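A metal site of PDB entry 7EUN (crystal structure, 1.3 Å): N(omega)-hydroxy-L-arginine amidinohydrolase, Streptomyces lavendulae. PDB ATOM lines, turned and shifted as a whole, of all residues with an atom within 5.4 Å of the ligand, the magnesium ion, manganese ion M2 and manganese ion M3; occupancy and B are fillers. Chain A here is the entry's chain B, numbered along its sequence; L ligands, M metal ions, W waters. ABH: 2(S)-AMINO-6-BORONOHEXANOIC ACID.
OG1 of Thr 122 is in hydrogen-bond range of O of the ligand.
The side-chain carboxylate of Asp 159 is in salt-bridge range of a nitrogen (N) of the ligand (2.8 Å).
An oxygen (OT) of the ligand lies within hydrogen-bond range of the side-chain amide nitrogen (ND2) of Asn 115, 3.1 Å away.
An oxygen (O2) of the ligand lies close to the backbone carbonyl oxygen of Gly 126 (3.5 Å).
N of the ligand is in salt-bridge range of OE1 of Glu 162 (3.9 Å).
N of Asp 113 is in hydrogen-bond range of OE2 of Glu 162, at 3.1 Å.
The side-chain carboxylate (OD2) of Asp 113 lies close to the side-chain hydroxyl (OH) of Tyr 107 (2.7 Å).
The side-chain carboxylate of Asp 200 lies close to the backbone NH of Gly 110, 3.1 Å away.
The side-chain sulfur of Cys 86 lies close to a ring nitrogen (NE2) of His 196 (3.3 Å).
The backbone NH (N) of Tyr 124 sits at hydrogen-bond distance from the side-chain hydroxyl (OG1) of Thr 122, 3.1 Å away.
The backbone NH (N) of Thr 122 sits at hydrogen-bond distance from the side-chain hydroxyl (OG1) of Thr 120 (3.4 Å).
The side-chain amide nitrogen of Asn 115 sits at hydrogen-bond distance from the side-chain carboxylate of Asp 159 (2.9 Å).
N of Asp 159 is in hydrogen-bond range of OE1 of Glu 162 (2.9 Å).
Residues that only touch the ligand: Tyr 124 (3.7 Å), Gly 127 (3.7 Å) and Tyr 211 (3.7 Å).
16 residues have an atom within 4 Å of the ligand: Cys 86, Asp 109, His 111, Asp 113, Asn 115, Thr 122, Tyr 124, Gly 126, Gly 127, Asp 159, Glu 162, Asp 198, Asp 200, Asp 210, Tyr 211 and Glu 241.
The nearest printed residue that does not touch the ligand is Thr 120 (4.4 Å).
Of the 22 residues printed, 4 come within 4 Å of the magnesium ion.
The nearest printed residue that does not touch the magnesium ion is Tyr 211 (4.3 Å).
Four residues have an atom within 4 Å of manganese ion M2: Cys 86, Asp 109, Asp 113 and Asp 198.
The nearest printed residue that does not touch manganese ion M2 is Tyr 107 (4.03 Å).
Four residues have an atom within 4 Å of manganese ion M3: Asp 109, His 111, Asp 198 and Asp 200.
The magnesium ion is bound by OE1 of Glu 241 (1.9 Å), OD1 of Asp 210 (2.0 Å), O3 of the ligand (2.2 Å), OD2 of Asp 200 (2.2 Å), OD2 of Asp 198 (2.3 Å) and OD1 of Asp 198 (2.5 Å).
Manganese ion M2 is bound by the side-chain carboxylate of Asp 109, an oxygen (O2) of the ligand, the side-chain carboxylate of Asp 113, an oxygen (O1) of the ligand, the side-chain carboxylate of Asp 198 and the side-chain sulfur of Cys 86.
Manganese ion M2 has six donor atoms within binding distance.
Manganese ion M3 is bound by O1 of the ligand, OD1 of Asp 109, OD2 of Asp 200, ND1 of His 111, OD2 of Asp 198 and OD1 of Asp 200.
Manganese ion M3 has six donor atoms within binding distance.
Slightly farther from manganese ion M3 lies O3 of the ligand (2.9 Å).
Water W5 bridges OH of Tyr 211 (2.5 Å) and O of the ligand (2.7 Å).
Water W1 lies within hydrogen-bond range of OG1 of Thr 120 (2.7 Å), OT of the ligand (2.7 Å) and O of Tyr 124 (2.8 Å).
Water W4 lies within hydrogen-bond range of OE2 of Glu 162 (2.7 Å), N of the ligand (2.8 Å), O of Gly 127 (2.8 Å), N of Asp 113 (3.3 Å) and ND2 of Asn 115 (3.4 Å).
Water W2 lies within hydrogen-bond range of OH of Tyr 124, OE2 of Glu 241 and OD2 of Asp 210.
Water W6 lies within hydrogen-bond range of OD1 of Asp 159, N of the ligand and OD1 of Asp 157.
Water W3 lies within hydrogen-bond range of the backbone carbonyl oxygen (O) of Asp 157 (2.7 Å), the side-chain carboxylate (OE1) of Glu 162 (2.8 Å) and a nitrogen (N) of the ligand (3.2 Å).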
ATOM      1  N   CYS A  86      12.386  19.549 -21.257  1.00  0.00           N
ATOM      2  CA  CYS A  86      12.965  18.366 -20.641  1.00  0.00           C
ATOM      3  C   CYS A  86      11.890  17.338 -20.267  1.00  0.00           C
ATOM      4  O   CYS A  86      12.181  16.147 -20.214  1.00  0.00           O
ATOM      5  CB  CYS A  86      13.788  18.740 -19.419  1.00  0.00           C
ATOM      6  SG  CYS A  86      15.344  19.544 -19.766  1.00  0.00           S
ATOM      7  N   TYR A 107      22.886  13.594 -17.959  1.00  0.00           N
ATOM      8  CA  TYR A 107      21.788  14.548 -17.863  1.00  0.00           C
ATOM      9  C   TYR A 107      22.440  15.914 -17.672  1.00  0.00           C
ATOM     10  O   TYR A 107      22.866  16.267 -16.566  1.00  0.00           O
ATOM     11  CB  TYR A 107      20.829  14.148 -16.750  1.00  0.00           C
ATOM     12  CG  TYR A 107      19.452  14.791 -16.870  1.00  0.00           C
ATOM     13  CD1 TYR A 107      19.246  16.105 -16.469  1.00  0.00           C
ATOM     14  CD2 TYR A 107      18.360  14.089 -17.386  1.00  0.00           C
ATOM     15  CE1 TYR A 107      17.987  16.695 -16.576  1.00  0.00           C
ATOM     16  CE2 TYR A 107      17.109  14.662 -17.481  1.00  0.00           C
ATOM     17  CZ  TYR A 107      16.930  15.965 -17.089  1.00  0.00           C
ATOM     18  OH  TYR A 107      15.664  16.512 -17.196  1.00  0.00           O
ATOM     19  N   ASP A 109      22.586  19.728 -17.612  1.00  0.00           N
ATOM     20  CA  ASP A 109      21.548  20.681 -17.224  1.00  0.00           C
ATOM     21  C   ASP A 109      22.132  21.608 -16.157  1.00  0.00           C
ATOM     22  O   ASP A 109      22.912  21.170 -15.319  1.00  0.00           O
ATOM     23  CB  ASP A 109      20.350  19.874 -16.676  1.00  0.00           C
ATOM     24  CG  ASP A 109      19.038  20.621 -16.693  1.00  0.00           C
ATOM     25  OD1 ASP A 109      18.989  21.779 -16.237  1.00  0.00           O
ATOM     26  OD2 ASP A 109      18.030  20.021 -17.150  1.00  0.00           O
ATOM     27  N   GLY A 110      21.715  22.880 -16.182  1.00  0.00           N
ATOM     28  CA  GLY A 110      22.069  23.784 -15.097  1.00  0.00           C
ATOM     29  C   GLY A 110      21.384  23.476 -13.782  1.00  0.00           C
ATOM     30  O   GLY A 110      21.810  23.977 -12.729  1.00  0.00           O
ATOM     31  N   HIS A 111      20.330  22.666 -13.834  1.00  0.00           N
ATOM     32  CA  HIS A 111      19.519  22.271 -12.692  1.00  0.00           C
ATOM     33  C   HIS A 111      19.688  20.771 -12.445  1.00  0.00           C
ATOM     34  O   HIS A 111      20.361  20.069 -13.199  1.00  0.00           O
ATOM     35  CB  HIS A 111      18.054  22.593 -12.984  1.00  0.00           C
ATOM     36  CG  HIS A 111      17.844  24.018 -13.332  1.00  0.00           C
ATOM     37  ND1 HIS A 111      17.721  24.468 -14.637  1.00  0.00           N
ATOM     38  CD2 HIS A 111      17.731  25.119 -12.547  1.00  0.00           C
ATOM     39  CE1 HIS A 111      17.555  25.774 -14.626  1.00  0.00           C
ATOM     40  NE2 HIS A 111      17.574  26.205 -13.377  1.00  0.00           N
ATOM     41  N   ASP A 113      16.756  18.770 -11.986  1.00  0.00           N
ATOM     42  CA  ASP A 113      15.505  18.151 -12.436  1.00  0.00           C
ATOM     43  C   ASP A 113      15.149  16.932 -11.587  1.00  0.00           C
ATOM     44  O   ASP A 113      14.652  15.929 -12.113  1.00  0.00           O
ATOM     45  CB  ASP A 113      15.519  17.832 -13.934  1.00  0.00           C
ATOM     46  CG  ASP A 113      15.611  19.077 -14.790  1.00  0.00           C
ATOM     47  OD1 ASP A 113      15.758  20.168 -14.204  1.00  0.00           O
ATOM     48  OD2 ASP A 113      15.555  18.979 -16.058  1.00  0.00           O
ATOM     49  N   ASN A 115      13.365  17.118  -8.337  1.00  0.00           N
ATOM     50  CA  ASN A 115      12.333  17.279  -7.332  1.00  0.00           C
ATOM     51  C   ASN A 115      11.229  16.221  -7.498  1.00  0.00           C
ATOM     52  O   ASN A 115      11.021  15.664  -8.575  1.00  0.00           O
ATOM     53  CB  ASN A 115      11.699  18.677  -7.418  1.00  0.00           C
ATOM     54  CG  ASN A 115      12.503  19.713  -6.688  1.00  0.00           C
ATOM     55  OD1 ASN A 115      12.777  19.560  -5.506  1.00  0.00           O
ATOM     56  ND2 ASN A 115      12.878  20.770  -7.372  1.00  0.00           N
ATOM     57  N   THR A 120       8.931  19.807  -4.611  1.00  0.00           N
ATOM     58  CA  THR A 120       8.845  20.958  -5.513  1.00  0.00           C
ATOM     59  C   THR A 120       8.210  22.143  -4.808  1.00  0.00           C
ATOM     60  O   THR A 120       7.202  22.005  -4.113  1.00  0.00           O
ATOM     61  CB  THR A 120       8.070  20.630  -6.784  1.00  0.00           C
ATOM     62  OG1 THR A 120       8.069  21.783  -7.638  1.00  0.00           O
ATOM     63  CG2 THR A 120       6.622  20.250  -6.512  1.00  0.00           C
ATOM     64  N   THR A 122       7.789  25.060  -6.916  1.00  0.00           N
ATOM     65  CA  THR A 122       7.221  25.757  -8.059  1.00  0.00           C
ATOM     66  C   THR A 122       6.097  24.981  -8.717  1.00  0.00           C
ATOM     67  O   THR A 122       5.355  25.559  -9.516  1.00  0.00           O
ATOM     68  CB  THR A 122       8.324  25.938  -9.108  1.00  0.00           C
ATOM     69  OG1 THR A 122       8.759  24.634  -9.511  1.00  0.00           O
ATOM     70  CG2 THR A 122       9.495  26.718  -8.553  1.00  0.00           C
ATOM     71  N   TYR A 124       6.644  22.903 -10.987  1.00  0.00           N
ATOM     72  CA  TYR A 124       7.008  22.795 -12.414  1.00  0.00           C
ATOM     73  C   TYR A 124       7.508  21.396 -12.738  1.00  0.00           C
ATOM     74  O   TYR A 124       8.522  20.949 -12.209  1.00  0.00           O
ATOM     75  CB  TYR A 124       8.051  23.828 -12.786  1.00  0.00           C
ATOM     76  CG  TYR A 124       8.427  23.789 -14.257  1.00  0.00           C
ATOM     77  CD1 TYR A 124       7.440  23.649 -15.241  1.00  0.00           C
ATOM     78  CD2 TYR A 124       9.846  23.850 -14.668  1.00  0.00           C
ATOM     79  CE1 TYR A 124       7.762  23.588 -16.572  1.00  0.00           C
ATOM     80  CE2 TYR A 124      10.187  23.730 -15.970  1.00  0.00           C
ATOM     81  CZ  TYR A 124       9.149  23.673 -16.934  1.00  0.00           C
ATOM     82  OH  TYR A 124       9.457  23.589 -18.246  1.00  0.00           O
ATOM     83  N   GLY A 126       9.053  20.283 -15.295  1.00  0.00           N
ATOM     84  CA  GLY A 126      10.400  20.204 -15.815  1.00  0.00           C
ATOM     85  C   GLY A 126      11.451  20.020 -14.746  1.00  0.00           C
ATOM     86  O   GLY A 126      12.528  19.480 -15.019  1.00  0.00           O
ATOM     87  N   GLY A 127      11.166  20.447 -13.523  1.00  0.00           N
ATOM     88  CA  GLY A 127      12.052  20.233 -12.398  1.00  0.00           C
ATOM     89  C   GLY A 127      11.954  18.877 -11.730  1.00  0.00           C
ATOM     90  O   GLY A 127      12.593  18.677 -10.691  1.00  0.00           O
ATOM     91  N   ASP A 157      22.348  25.041  -9.925  1.00  0.00           N
ATOM     92  CA  ASP A 157      21.221  25.679  -9.233  1.00  0.00           C
ATOM     93  C   ASP A 157      20.284  24.549  -8.794  1.00  0.00           C
ATOM     94  O   ASP A 157      19.408  24.141  -9.542  1.00  0.00           O
ATOM     95  CB  ASP A 157      20.538  26.698 -10.135  1.00  0.00           C
ATOM     96  CG  ASP A 157      19.462  27.486  -9.409  1.00  0.00           C
ATOM     97  OD1 ASP A 157      19.090  27.078  -8.291  1.00  0.00           O
ATOM     98  OD2 ASP A 157      18.996  28.525  -9.947  1.00  0.00           O
ATOM     99  N   ASP A 159      17.847  22.943  -5.643  1.00  0.00           N
ATOM    100  CA  ASP A 159      17.058  23.311  -4.467  1.00  0.00           C
ATOM    101  C   ASP A 159      17.515  22.480  -3.251  1.00  0.00           C
ATOM    102  O   ASP A 159      18.153  21.445  -3.373  1.00  0.00           O
ATOM    103  CB  ASP A 159      15.568  23.112  -4.729  1.00  0.00           C
ATOM    104  CG  ASP A 159      15.085  23.844  -5.971  1.00  0.00           C
ATOM    105  OD1 ASP A 159      15.530  24.991  -6.207  1.00  0.00           O
ATOM    106  OD2 ASP A 159      14.232  23.284  -6.696  1.00  0.00           O
ATOM    107  N   GLU A 162      15.862  19.059  -2.987  1.00  0.00           N
ATOM    108  CA  GLU A 162      16.334  18.342  -4.169  1.00  0.00           C
ATOM    109  C   GLU A 162      17.766  17.835  -3.986  1.00  0.00           C
ATOM    110  O   GLU A 162      18.073  16.697  -4.366  1.00  0.00           O
ATOM    111  CB  GLU A 162      16.273  19.317  -5.360  1.00  0.00           C
ATOM    112  CG  GLU A 162      16.639  18.736  -6.696  1.00  0.00           C
ATOM    113  CD  GLU A 162      16.646  19.766  -7.816  1.00  0.00           C
ATOM    114  OE1 GLU A 162      16.774  20.980  -7.515  1.00  0.00           O
ATOM    115  OE2 GLU A 162      16.546  19.357  -8.995  1.00  0.00           O
ATOM    116  N   HIS A 196      21.288  13.635 -22.657  1.00  0.00           N
ATOM    117  CA  HIS A 196      20.147  14.554 -22.541  1.00  0.00           C
ATOM    118  C   HIS A 196      20.685  15.929 -22.226  1.00  0.00           C
ATOM    119  O   HIS A 196      21.355  16.088 -21.203  1.00  0.00           O
ATOM    120  CB  HIS A 196      19.213  14.093 -21.416  1.00  0.00           C
ATOM    121  CG  HIS A 196      18.132  15.068 -21.050  1.00  0.00           C
ATOM    122  ND1 HIS A 196      16.800  14.822 -21.318  1.00  0.00           N
ATOM    123  CD2 HIS A 196      18.180  16.270 -20.421  1.00  0.00           C
ATOM    124  CE1 HIS A 196      16.079  15.852 -20.890  1.00  0.00           C
ATOM    125  NE2 HIS A 196      16.884  16.736 -20.344  1.00  0.00           N
ATOM    126  N   ASP A 198      19.798  20.099 -21.694  1.00  0.00           N
ATOM    127  CA  ASP A 198      19.002  21.313 -21.523  1.00  0.00           C
ATOM    128  C   ASP A 198      19.936  22.493 -21.723  1.00  0.00           C
ATOM    129  O   ASP A 198      20.942  22.612 -21.005  1.00  0.00           O
ATOM    130  CB  ASP A 198      18.430  21.273 -20.099  1.00  0.00           C
ATOM    131  CG  ASP A 198      17.647  22.520 -19.650  1.00  0.00           C
ATOM    132  OD1 ASP A 198      17.672  23.562 -20.316  1.00  0.00           O
ATOM    133  OD2 ASP A 198      16.976  22.384 -18.583  1.00  0.00           O
ATOM    134  N   ASP A 200      20.003  25.417 -20.871  1.00  0.00           N
ATOM    135  CA  ASP A 200      20.305  26.278 -19.720  1.00  0.00           C
ATOM    136  C   ASP A 200      21.575  25.840 -18.973  1.00  0.00           C
ATOM    137  O   ASP A 200      22.028  26.561 -18.082  1.00  0.00           O
ATOM    138  CB  ASP A 200      19.090  26.480 -18.813  1.00  0.00           C
ATOM    139  CG  ASP A 200      18.667  25.246 -18.010  1.00  0.00           C
ATOM    140  OD1 ASP A 200      19.492  24.396 -17.656  1.00  0.00           O
ATOM    141  OD2 ASP A 200      17.452  25.174 -17.692  1.00  0.00           O
ATOM    142  N   ALA A 209      17.667  30.083 -23.315  1.00  0.00           N
ATOM    143  CA  ALA A 209      16.973  28.936 -22.766  1.00  0.00           C
ATOM    144  C   ALA A 209      15.816  29.410 -21.888  1.00  0.00           C
ATOM    145  O   ALA A 209      15.455  30.578 -21.883  1.00  0.00           O
ATOM    146  CB  ALA A 209      17.951  28.008 -22.047  1.00  0.00           C
ATOM    147  N   ASP A 210      15.204  28.470 -21.177  1.00  0.00           N
ATOM    148  CA  ASP A 210      14.087  28.836 -20.316  1.00  0.00           C
ATOM    149  C   ASP A 210      14.531  29.479 -19.003  1.00  0.00           C
ATOM    150  O   ASP A 210      13.726  30.177 -18.371  1.00  0.00           O
ATOM    151  CB  ASP A 210      13.190  27.614 -20.085  1.00  0.00           C
ATOM    152  CG  ASP A 210      13.875  26.468 -19.330  1.00  0.00           C
ATOM    153  OD1 ASP A 210      15.132  26.205 -19.439  1.00  0.00           O
ATOM    154  OD2 ASP A 210      13.096  25.800 -18.609  1.00  0.00           O
ATOM    155  N   TYR A 211      15.766  29.272 -18.591  1.00  0.00           N
ATOM    156  CA  TYR A 211      16.366  29.928 -17.408  1.00  0.00           C
ATOM    157  C   TYR A 211      17.744  30.453 -17.838  1.00  0.00           C
ATOM    158  O   TYR A 211      18.404  29.869 -18.716  1.00  0.00           O
ATOM    159  CB  TYR A 211      16.571  28.980 -16.223  1.00  0.00           C
ATOM    160  CG  TYR A 211      15.303  28.502 -15.618  1.00  0.00           C
ATOM    161  CD1 TYR A 211      14.802  29.070 -14.440  1.00  0.00           C
ATOM    162  CD2 TYR A 211      14.543  27.488 -16.242  1.00  0.00           C
ATOM    163  CE1 TYR A 211      13.604  28.631 -13.877  1.00  0.00           C
ATOM    164  CE2 TYR A 211      13.396  27.063 -15.716  1.00  0.00           C
ATOM    165  CZ  TYR A 211      12.912  27.617 -14.537  1.00  0.00           C
ATOM    166  OH  TYR A 211      11.711  27.096 -14.050  1.00  0.00           O
ATOM    167  N   GLU A 241      15.093  22.678 -25.004  1.00  0.00           N
ATOM    168  CA  GLU A 241      14.906  23.962 -24.299  1.00  0.00           C
ATOM    169  C   GLU A 241      15.609  25.152 -24.945  1.00  0.00           C
ATOM    170  O   GLU A 241      16.083  26.025 -24.254  1.00  0.00           O
ATOM    171  CB  GLU A 241      15.179  23.827 -22.797  1.00  0.00           C
ATOM    172  CG  GLU A 241      14.458  22.616 -22.213  1.00  0.00           C
ATOM    173  CD  GLU A 241      13.877  22.809 -20.872  1.00  0.00           C
ATOM    174  OE1 GLU A 241      14.458  23.527 -20.072  1.00  0.00           O
ATOM    175  OE2 GLU A 241      12.808  22.221 -20.591  1.00  0.00           O
HETATM  176  N   ABH L   1      14.517  23.397  -9.517  1.00  0.00           N
HETATM  177  CA  ABH L   1      13.575  24.361 -10.172  1.00  0.00           C
HETATM  178  C   ABH L   1      12.153  23.895 -10.088  1.00  0.00           C
HETATM  179  O   ABH L   1      11.245  24.651 -10.510  1.00  0.00           O
HETATM  180  OT  ABH L   1      11.909  22.828  -9.474  1.00  0.00           O
HETATM  181  CB  ABH L   1      14.015  24.658 -11.597  1.00  0.00           C
HETATM  182  CG  ABH L   1      13.611  23.580 -12.614  1.00  0.00           C
HETATM  183  CD  ABH L   1      14.226  23.811 -14.007  1.00  0.00           C
HETATM  184  CE  ABH L   1      13.654  22.866 -15.049  1.00  0.00           C
HETATM  185  B   ABH L   1      14.594  22.556 -16.284  1.00  0.00           B
HETATM  186  O2  ABH L   1      14.094  21.563 -17.283  1.00  0.00           O
HETATM  187  O1  ABH L   1      15.983  22.151 -15.979  1.00  0.00           O
HETATM  188  O3  ABH L   1      14.809  23.873 -17.063  1.00  0.00           O
HETATM  189 MG    MG M   1      15.797  24.340 -18.938  1.00  0.00          MG
HETATM  190 MN    MN M   2      15.985  20.513 -17.568  1.00  0.00          MN
HETATM  191 MN    MN M   3      17.596  23.321 -16.513  1.00  0.00          MN
HETATM  192  O   HOH W   1       9.696  21.242  -9.663  1.00  0.00           O
HETATM  193  O   HOH W   2      12.036  23.400 -18.387  1.00  0.00           O
HETATM  194  O   HOH W   3      17.449  22.279  -9.850  1.00  0.00           O
HETATM  195  O   HOH W   4      14.584  20.682 -10.328  1.00  0.00           O
HETATM  196  O   HOH W   5      11.236  27.122 -11.579  1.00  0.00           O
HETATM  197  O   HOH W   6      16.519  25.497  -8.857  1.00  0.00           O
HETATM  198  O   HOH W   7      11.088  23.789  -6.790  1.00  0.00           O
